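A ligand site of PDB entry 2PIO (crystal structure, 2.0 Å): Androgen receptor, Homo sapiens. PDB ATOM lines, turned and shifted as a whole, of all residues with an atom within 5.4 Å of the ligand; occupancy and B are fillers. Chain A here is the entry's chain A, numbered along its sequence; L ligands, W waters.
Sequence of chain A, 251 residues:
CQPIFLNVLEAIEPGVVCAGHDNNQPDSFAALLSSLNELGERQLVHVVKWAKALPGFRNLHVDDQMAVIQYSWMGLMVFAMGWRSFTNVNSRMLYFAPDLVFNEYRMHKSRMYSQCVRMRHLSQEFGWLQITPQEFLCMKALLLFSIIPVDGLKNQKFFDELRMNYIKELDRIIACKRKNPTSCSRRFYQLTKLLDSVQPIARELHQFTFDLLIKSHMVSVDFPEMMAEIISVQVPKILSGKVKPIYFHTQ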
ATOM      1  N   LEU A  33     -31.051  12.414 -17.543  1.00  0.00           N
ATOM      2  CA  LEU A  33     -30.398  13.206 -16.514  1.00  0.00           C
ATOM      3  C   LEU A  33     -30.165  12.397 -15.259  1.00  0.00           C
ATOM      4  O   LEU A  33     -29.150  12.569 -14.581  1.00  0.00           O
ATOM      5  CB  LEU A  33     -31.209  14.465 -16.198  1.00  0.00           C
ATOM      6  CG  LEU A  33     -30.730  15.689 -17.002  1.00  0.00           C
ATOM      7  CD1 LEU A  33     -29.279  15.990 -16.659  1.00  0.00           C
ATOM      8  CD2 LEU A  33     -30.896  15.436 -18.493  1.00  0.00           C
ATOM      9  N   LEU A  36     -27.099  10.385 -16.074  1.00  0.00           N
ATOM     10  CA  LEU A  36     -25.885  11.204 -16.076  1.00  0.00           C
ATOM     11  C   LEU A  36     -25.455  11.480 -14.644  1.00  0.00           C
ATOM     12  O   LEU A  36     -24.266  11.483 -14.331  1.00  0.00           O
ATOM     13  CB  LEU A  36     -26.129  12.531 -16.793  1.00  0.00           C
ATOM     14  CG  LEU A  36     -26.082  12.541 -18.323  1.00  0.00           C
ATOM     15  CD1 LEU A  36     -26.601  13.885 -18.818  1.00  0.00           C
ATOM     16  CD2 LEU A  36     -24.655  12.291 -18.821  1.00  0.00           C
ATOM     17  N   ASN A  37     -26.437  11.713 -13.771  1.00  0.00           N
ATOM     18  CA  ASN A  37     -26.175  11.984 -12.362  1.00  0.00           C
ATOM     19  C   ASN A  37     -25.565  10.796 -11.645  1.00  0.00           C
ATOM     20  O   ASN A  37     -24.616  10.946 -10.852  1.00  0.00           O
ATOM     21  CB  ASN A  37     -27.460  12.401 -11.651  1.00  0.00           C
ATOM     22  CG  ASN A  37     -27.825  13.846 -11.947  1.00  0.00           C
ATOM     23  OD1 ASN A  37     -26.945  14.707 -12.116  1.00  0.00           O
ATOM     24  ND2 ASN A  37     -29.120  14.143 -11.992  1.00  0.00           N
ATOM     25  N   LEU A  39     -23.953   8.496 -13.058  1.00  0.00           N
ATOM     26  CA  LEU A  39     -22.634   8.390 -13.646  1.00  0.00           C
ATOM     27  C   LEU A  39     -21.687   9.336 -12.913  1.00  0.00           C
ATOM     28  O   LEU A  39     -20.492   9.055 -12.759  1.00  0.00           O
ATOM     29  CB  LEU A  39     -22.689   8.755 -15.135  1.00  0.00           C
ATOM     30  CG  LEU A  39     -21.335   8.650 -15.873  1.00  0.00           C
ATOM     31  CD1 LEU A  39     -20.785   7.223 -15.768  1.00  0.00           C
ATOM     32  CD2 LEU A  39     -21.485   9.046 -17.310  1.00  0.00           C
ATOM     33  N   GLY A  40     -22.214  10.472 -12.471  1.00  0.00           N
ATOM     34  CA  GLY A  40     -21.399  11.449 -11.740  1.00  0.00           C
ATOM     35  C   GLY A  40     -20.991  10.866 -10.395  1.00  0.00           C
ATOM     36  O   GLY A  40     -19.826  10.949 -10.004  1.00  0.00           O
ATOM     37  N   GLN A  43     -18.462   8.152 -11.090  1.00  0.00           N
ATOM     38  CA  GLN A  43     -17.209   8.773 -11.509  1.00  0.00           C
ATOM     39  C   GLN A  43     -16.484   9.504 -10.376  1.00  0.00           C
ATOM     40  O   GLN A  43     -15.251   9.466 -10.283  1.00  0.00           O
ATOM     41  CB  GLN A  43     -17.446   9.759 -12.660  1.00  0.00           C
ATOM     42  CG  GLN A  43     -17.559   9.105 -14.034  1.00  0.00           C
ATOM     43  CD  GLN A  43     -16.265   8.438 -14.459  1.00  0.00           C
ATOM     44  OE1 GLN A  43     -16.211   7.761 -15.500  1.00  0.00           O
ATOM     45  NE2 GLN A  43     -15.222   8.615 -13.662  1.00  0.00           N
ATOM     46  N   TRP A  73     -14.196  18.596  -9.971  1.00  0.00           N
ATOM     47  CA  TRP A  73     -14.718  17.381 -10.602  1.00  0.00           C
ATOM     48  C   TRP A  73     -15.406  17.619 -11.947  1.00  0.00           C
ATOM     49  O   TRP A  73     -15.201  16.850 -12.892  1.00  0.00           O
ATOM     50  CB  TRP A  73     -15.667  16.635  -9.647  1.00  0.00           C
ATOM     51  CG  TRP A  73     -16.861  17.417  -9.234  1.00  0.00           C
ATOM     52  CD1 TRP A  73     -16.917  18.347  -8.240  1.00  0.00           C
ATOM     53  CD2 TRP A  73     -18.159  17.404  -9.841  1.00  0.00           C
ATOM     54  NE1 TRP A  73     -18.162  18.918  -8.183  1.00  0.00           N
ATOM     55  CE2 TRP A  73     -18.952  18.358  -9.154  1.00  0.00           C
ATOM     56  CE3 TRP A  73     -18.725  16.671 -10.894  1.00  0.00           C
ATOM     57  CZ2 TRP A  73     -20.282  18.598  -9.486  1.00  0.00           C
ATOM     58  CZ3 TRP A  73     -20.060  16.920 -11.227  1.00  0.00           C
ATOM     59  CH2 TRP A  73     -20.824  17.881 -10.527  1.00  0.00           C
ATOM     60  N   MET A  74     -16.213  18.668 -12.054  1.00  0.00           N
ATOM     61  CA  MET A  74     -16.908  18.947 -13.300  1.00  0.00           C
ATOM     62  C   MET A  74     -15.940  19.057 -14.481  1.00  0.00           C
ATOM     63  O   MET A  74     -16.070  18.328 -15.472  1.00  0.00           O
ATOM     64  CB  MET A  74     -17.719  20.257 -13.190  1.00  0.00           C
ATOM     65  CG  MET A  74     -18.649  20.522 -14.365  1.00  0.00           C
ATOM     66  SD  MET A  74     -19.981  19.286 -14.522  1.00  0.00           S
ATOM     67  CE  MET A  74     -21.262  19.954 -13.376  1.00  0.00           C
ATOM     68  N   MET A  77     -14.062  15.687 -15.202  1.00  0.00           N
ATOM     69  CA  MET A  77     -14.949  14.733 -15.867  1.00  0.00           C
ATOM     70  C   MET A  77     -15.301  15.125 -17.296  1.00  0.00           C
ATOM     71  O   MET A  77     -15.333  14.268 -18.197  1.00  0.00           O
ATOM     72  CB  MET A  77     -16.237  14.568 -15.042  1.00  0.00           C
ATOM     73  CG  MET A  77     -16.037  13.917 -13.675  1.00  0.00           C
ATOM     74  SD  MET A  77     -17.596  13.496 -12.866  1.00  0.00           S
ATOM     75  CE  MET A  77     -17.061  13.176 -11.203  1.00  0.00           C
ATOM     76  N   VAL A  78     -15.558  16.402 -17.516  1.00  0.00           N
ATOM     77  CA  VAL A  78     -15.911  16.877 -18.848  1.00  0.00           C
ATOM     78  C   VAL A  78     -14.727  16.733 -19.806  1.00  0.00           C
ATOM     79  O   VAL A  78     -14.885  16.336 -20.956  1.00  0.00           O
ATOM     80  CB  VAL A  78     -16.374  18.350 -18.808  1.00  0.00           C
ATOM     81  CG1 VAL A  78     -16.561  18.877 -20.231  1.00  0.00           C
ATOM     82  CG2 VAL A  78     -17.675  18.441 -18.050  1.00  0.00           C
ATOM     83  N   MET A  81     -14.232  13.142 -20.597  1.00  0.00           N
ATOM     84  CA  MET A  81     -15.350  12.709 -21.424  1.00  0.00           C
ATOM     85  C   MET A  81     -15.078  13.112 -22.875  1.00  0.00           C
ATOM     86  O   MET A  81     -15.329  12.350 -23.797  1.00  0.00           O
ATOM     87  CB  MET A  81     -16.660  13.328 -20.927  1.00  0.00           C
ATOM     88  CG  MET A  81     -17.915  12.839 -21.656  1.00  0.00           C
ATOM     89  SD  MET A  81     -18.183  13.639 -23.285  1.00  0.00           S
ATOM     90  CE  MET A  81     -18.620  15.318 -22.761  1.00  0.00           C
ATOM     91  N   ARG A  84     -12.584  10.661 -24.400  1.00  0.00           N
ATOM     92  CA  ARG A  84     -13.214   9.383 -24.779  1.00  0.00           C
ATOM     93  C   ARG A  84     -14.017   9.542 -26.077  1.00  0.00           C
ATOM     94  O   ARG A  84     -14.025   8.664 -26.943  1.00  0.00           O
ATOM     95  CB  ARG A  84     -14.182   8.912 -23.707  1.00  0.00           C
ATOM     96  CG  ARG A  84     -13.575   8.476 -22.406  1.00  0.00           C
ATOM     97  CD  ARG A  84     -14.593   7.696 -21.590  1.00  0.00           C
ATOM     98  NE  ARG A  84     -15.695   8.515 -21.060  1.00  0.00           N
ATOM     99  CZ  ARG A  84     -15.590   9.348 -20.020  1.00  0.00           C
ATOM    100  NH1 ARG A  84     -14.432   9.483 -19.375  1.00  0.00           N
ATOM    101  NH2 ARG A  84     -16.653  10.014 -19.596  1.00  0.00           N
ATOM    102  N   PHE A  96     -20.258   9.605 -22.892  1.00  0.00           N
ATOM    103  CA  PHE A  96     -20.217   9.751 -21.445  1.00  0.00           C
ATOM    104  C   PHE A  96     -19.786   8.419 -20.806  1.00  0.00           C
ATOM    105  O   PHE A  96     -18.947   8.385 -19.907  1.00  0.00           O
ATOM    106  CB  PHE A  96     -21.600  10.151 -20.915  1.00  0.00           C
ATOM    107  CG  PHE A  96     -22.034  11.539 -21.307  1.00  0.00           C
ATOM    108  CD1 PHE A  96     -21.458  12.658 -20.726  1.00  0.00           C
ATOM    109  CD2 PHE A  96     -23.022  11.715 -22.273  1.00  0.00           C
ATOM    110  CE1 PHE A  96     -21.869  13.953 -21.082  1.00  0.00           C
ATOM    111  CE2 PHE A  96     -23.445  13.001 -22.643  1.00  0.00           C
ATOM    112  CZ  PHE A  96     -22.863  14.124 -22.041  1.00  0.00           C
ATOM    113  N   MET A 112     -30.133  20.239 -22.629  1.00  0.00           N
ATOM    114  CA  MET A 112     -28.858  20.916 -22.440  1.00  0.00           C
ATOM    115  C   MET A 112     -28.055  20.759 -23.711  1.00  0.00           C
ATOM    116  O   MET A 112     -26.865  20.477 -23.685  1.00  0.00           O
ATOM    117  CB  MET A 112     -28.096  20.357 -21.235  1.00  0.00           C
ATOM    118  CG  MET A 112     -27.890  18.866 -21.195  1.00  0.00           C
ATOM    119  SD  MET A 112     -26.881  18.411 -19.759  1.00  0.00           S
ATOM    120  CE  MET A 112     -25.298  18.052 -20.551  1.00  0.00           C
ATOM    121  N   MET A 119     -19.382  20.874 -25.304  1.00  0.00           N
ATOM    122  CA  MET A 119     -18.547  19.720 -25.000  1.00  0.00           C
ATOM    123  C   MET A 119     -18.051  18.970 -26.231  1.00  0.00           C
ATOM    124  O   MET A 119     -16.930  18.460 -26.242  1.00  0.00           O
ATOM    125  CB  MET A 119     -19.288  18.765 -24.063  1.00  0.00           C
ATOM    126  CG  MET A 119     -19.494  19.360 -22.677  1.00  0.00           C
ATOM    127  SD  MET A 119     -20.228  18.261 -21.470  1.00  0.00           S
ATOM    128  CE  MET A 119     -21.994  18.341 -21.977  1.00  0.00           C
ATOM    129  N   LEU A 205     -22.140  24.117 -17.058  1.00  0.00           N
ATOM    130  CA  LEU A 205     -22.696  22.903 -16.500  1.00  0.00           C
ATOM    131  C   LEU A 205     -23.041  23.053 -15.018  1.00  0.00           C
ATOM    132  O   LEU A 205     -24.015  22.488 -14.560  1.00  0.00           O
ATOM    133  CB  LEU A 205     -21.730  21.724 -16.723  1.00  0.00           C
ATOM    134  CG  LEU A 205     -21.622  21.256 -18.185  1.00  0.00           C
ATOM    135  CD1 LEU A 205     -20.581  20.162 -18.306  1.00  0.00           C
ATOM    136  CD2 LEU A 205     -22.985  20.752 -18.677  1.00  0.00           C
ATOM    137  N   PHE A 208     -26.301  24.821 -14.824  1.00  0.00           N
ATOM    138  CA  PHE A 208     -27.358  23.895 -15.235  1.00  0.00           C
ATOM    139  C   PHE A 208     -27.703  22.855 -14.177  1.00  0.00           C
ATOM    140  O   PHE A 208     -28.869  22.668 -13.830  1.00  0.00           O
ATOM    141  CB  PHE A 208     -26.973  23.190 -16.541  1.00  0.00           C
ATOM    142  CG  PHE A 208     -28.057  22.320 -17.108  1.00  0.00           C
ATOM    143  CD1 PHE A 208     -28.216  21.014 -16.676  1.00  0.00           C
ATOM    144  CD2 PHE A 208     -28.934  22.824 -18.076  1.00  0.00           C
ATOM    145  CE1 PHE A 208     -29.227  20.204 -17.183  1.00  0.00           C
ATOM    146  CE2 PHE A 208     -29.957  22.030 -18.596  1.00  0.00           C
ATOM    147  CZ  PHE A 208     -30.110  20.716 -18.150  1.00  0.00           C
ATOM    148  N   THR A 209     -26.695  22.166 -13.644  1.00  0.00           N
ATOM    149  CA  THR A 209     -26.977  21.157 -12.630  1.00  0.00           C
ATOM    150  C   THR A 209     -27.545  21.775 -11.359  1.00  0.00           C
ATOM    151  O   THR A 209     -28.349  21.152 -10.666  1.00  0.00           O
ATOM    152  CB  THR A 209     -25.707  20.322 -12.288  1.00  0.00           C
ATOM    153  OG1 THR A 209     -26.088  19.177 -11.531  1.00  0.00           O
ATOM    154  CG2 THR A 209     -24.702  21.161 -11.484  1.00  0.00           C
ATOM    155  N   LEU A 212     -31.046  22.373 -11.912  1.00  0.00           N
ATOM    156  CA  LEU A 212     -31.667  21.063 -11.987  1.00  0.00           C
ATOM    157  C   LEU A 212     -31.921  20.479 -10.591  1.00  0.00           C
ATOM    158  O   LEU A 212     -32.972  19.876 -10.349  1.00  0.00           O
ATOM    159  CB  LEU A 212     -30.779  20.102 -12.784  1.00  0.00           C
ATOM    160  CG  LEU A 212     -31.368  18.718 -13.064  1.00  0.00           C
ATOM    161  CD1 LEU A 212     -32.717  18.852 -13.741  1.00  0.00           C
ATOM    162  CD2 LEU A 212     -30.415  17.934 -13.935  1.00  0.00           C
ATOM    163  N   PHE A 223     -30.834  12.704  -7.931  1.00  0.00           N
ATOM    164  CA  PHE A 223     -29.463  13.108  -7.622  1.00  0.00           C
ATOM    165  C   PHE A 223     -29.004  12.223  -6.466  1.00  0.00           C
ATOM    166  O   PHE A 223     -29.645  12.178  -5.410  1.00  0.00           O
ATOM    167  CB  PHE A 223     -29.392  14.574  -7.162  1.00  0.00           C
ATOM    168  CG  PHE A 223     -29.402  15.580  -8.293  1.00  0.00           C
ATOM    169  CD1 PHE A 223     -30.603  15.994  -8.873  1.00  0.00           C
ATOM    170  CD2 PHE A 223     -28.215  16.145  -8.751  1.00  0.00           C
ATOM    171  CE1 PHE A 223     -30.617  16.961  -9.890  1.00  0.00           C
ATOM    172  CE2 PHE A 223     -28.211  17.111  -9.769  1.00  0.00           C
ATOM    173  CZ  PHE A 223     -29.412  17.512 -10.341  1.00  0.00           C
ATOM    174  N   ILE A 231     -23.325  19.672  -5.009  1.00  0.00           N
ATOM    175  CA  ILE A 231     -23.949  20.695  -5.836  1.00  0.00           C
ATOM    176  C   ILE A 231     -24.702  21.735  -5.031  1.00  0.00           C
ATOM    177  O   ILE A 231     -24.930  22.841  -5.498  1.00  0.00           O
ATOM    178  CB  ILE A 231     -24.894  20.044  -6.878  1.00  0.00           C
ATOM    179  CG1 ILE A 231     -24.095  19.071  -7.749  1.00  0.00           C
ATOM    180  CG2 ILE A 231     -25.547  21.120  -7.740  1.00  0.00           C
ATOM    181  CD1 ILE A 231     -24.938  18.259  -8.728  1.00  0.00           C
HETATM  182  C1  LIG L   1     -20.823  12.819 -15.754  1.00  0.00           C
HETATM  183  C2  LIG L   1     -19.413  12.314 -16.086  1.00  0.00           C
HETATM  184  C3  LIG L   1     -19.129  12.750 -17.552  1.00  0.00           C
HETATM  185  O1  LIG L   1     -18.770  11.914 -18.346  1.00  0.00           O
HETATM  186  C4  LIG L   1     -19.341  14.191 -17.896  1.00  0.00           C
HETATM  187  C5  LIG L   1     -20.781  14.639 -17.562  1.00  0.00           C
HETATM  188  C6  LIG L   1     -21.049  16.139 -17.905  1.00  0.00           C
HETATM  189  C7  LIG L   1     -22.503  16.506 -17.556  1.00  0.00           C
HETATM  190  C8  LIG L   1     -22.849  16.268 -16.048  1.00  0.00           C
HETATM  191  C9  LIG L   1     -22.576  14.760 -15.705  1.00  0.00           C
HETATM  192  C10 LIG L   1     -21.082  14.336 -16.012  1.00  0.00           C
HETATM  193  C11 LIG L   1     -22.976  14.524 -14.209  1.00  0.00           C
HETATM  194  C12 LIG L   1     -24.392  14.927 -13.812  1.00  0.00           C
HETATM  195  C13 LIG L   1     -24.744  16.383 -14.230  1.00  0.00           C
HETATM  196  C14 LIG L   1     -24.328  16.594 -15.740  1.00  0.00           C
HETATM  197  C15 LIG L   1     -24.802  18.038 -15.997  1.00  0.00           C
HETATM  198  C16 LIG L   1     -26.189  18.049 -15.320  1.00  0.00           C
HETATM  199  C17 LIG L   1     -26.203  16.787 -14.411  1.00  0.00           C
HETATM  200  O2  LIG L   1     -26.865  17.125 -13.183  1.00  0.00           O
HETATM  201  C18 LIG L   1     -23.984  17.380 -13.257  1.00  0.00           C
HETATM  202  C19 LIG L   1     -20.108  15.177 -15.094  1.00  0.00           C
HETATM  203  O   HOH W   1     -15.660  11.527 -17.039  1.00  0.00           O
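ND2 of Asn 37 lies within hydrogen-bond range of O of Leu 33 (3.0 Å).
O of Phe 96 sits at hydrogen-bond distance from NH2 of Arg 84 (2.8 Å).
Water W1 lies within hydrogen-bond range of the backbone carbonyl oxygen (O) of Met 77 (3.0 Å), the guanidinium group (NH2) of Arg 84 (3.1 Å) and an oxygen (O1) of the ligand (3.4 Å).
An oxygen (O2) of the ligand is in hydrogen-bond range of the side-chain amide oxygen (OD1) of Asn 37, at 2.6 Å.
O2 of the ligand is in hydrogen-bond range of OG1 of Thr 209, 2.7 Å away.
NH2 of Arg 84 lies within hydrogen-bond range of O1 of the ligand, at 3.1 Å.
Leu 33 touches the ligand.
Leu 36 touches the ligand (O to C11, 3.3 Å).
CE of Met 74 touches C18 of the ligand, at 3.7 Å.
Met 77 touches the ligand (SD to C19, 3.8 Å).
Met 81 touches the ligand (CG to O1, 3.5 Å).
CD1 of Phe 96 touches O1 of the ligand, at 3.7 Å.
Phe 208 touches the ligand.
Leu 212 touches the ligand (CD2 to O2, 3.7 Å).
CE2 of Phe 223 touches O2 of the ligand, 3.7 Å away.
Within 4 Å of the ligand: Leu 33, Leu 36, Asn 37, Met 74, Met 77, Met 81, Arg 84, Phe 96, Phe 208, Thr 209, Leu 212 and Phe 223.
The nearest printed residue that does not touch the ligand is Leu 39 (4.1 Å).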
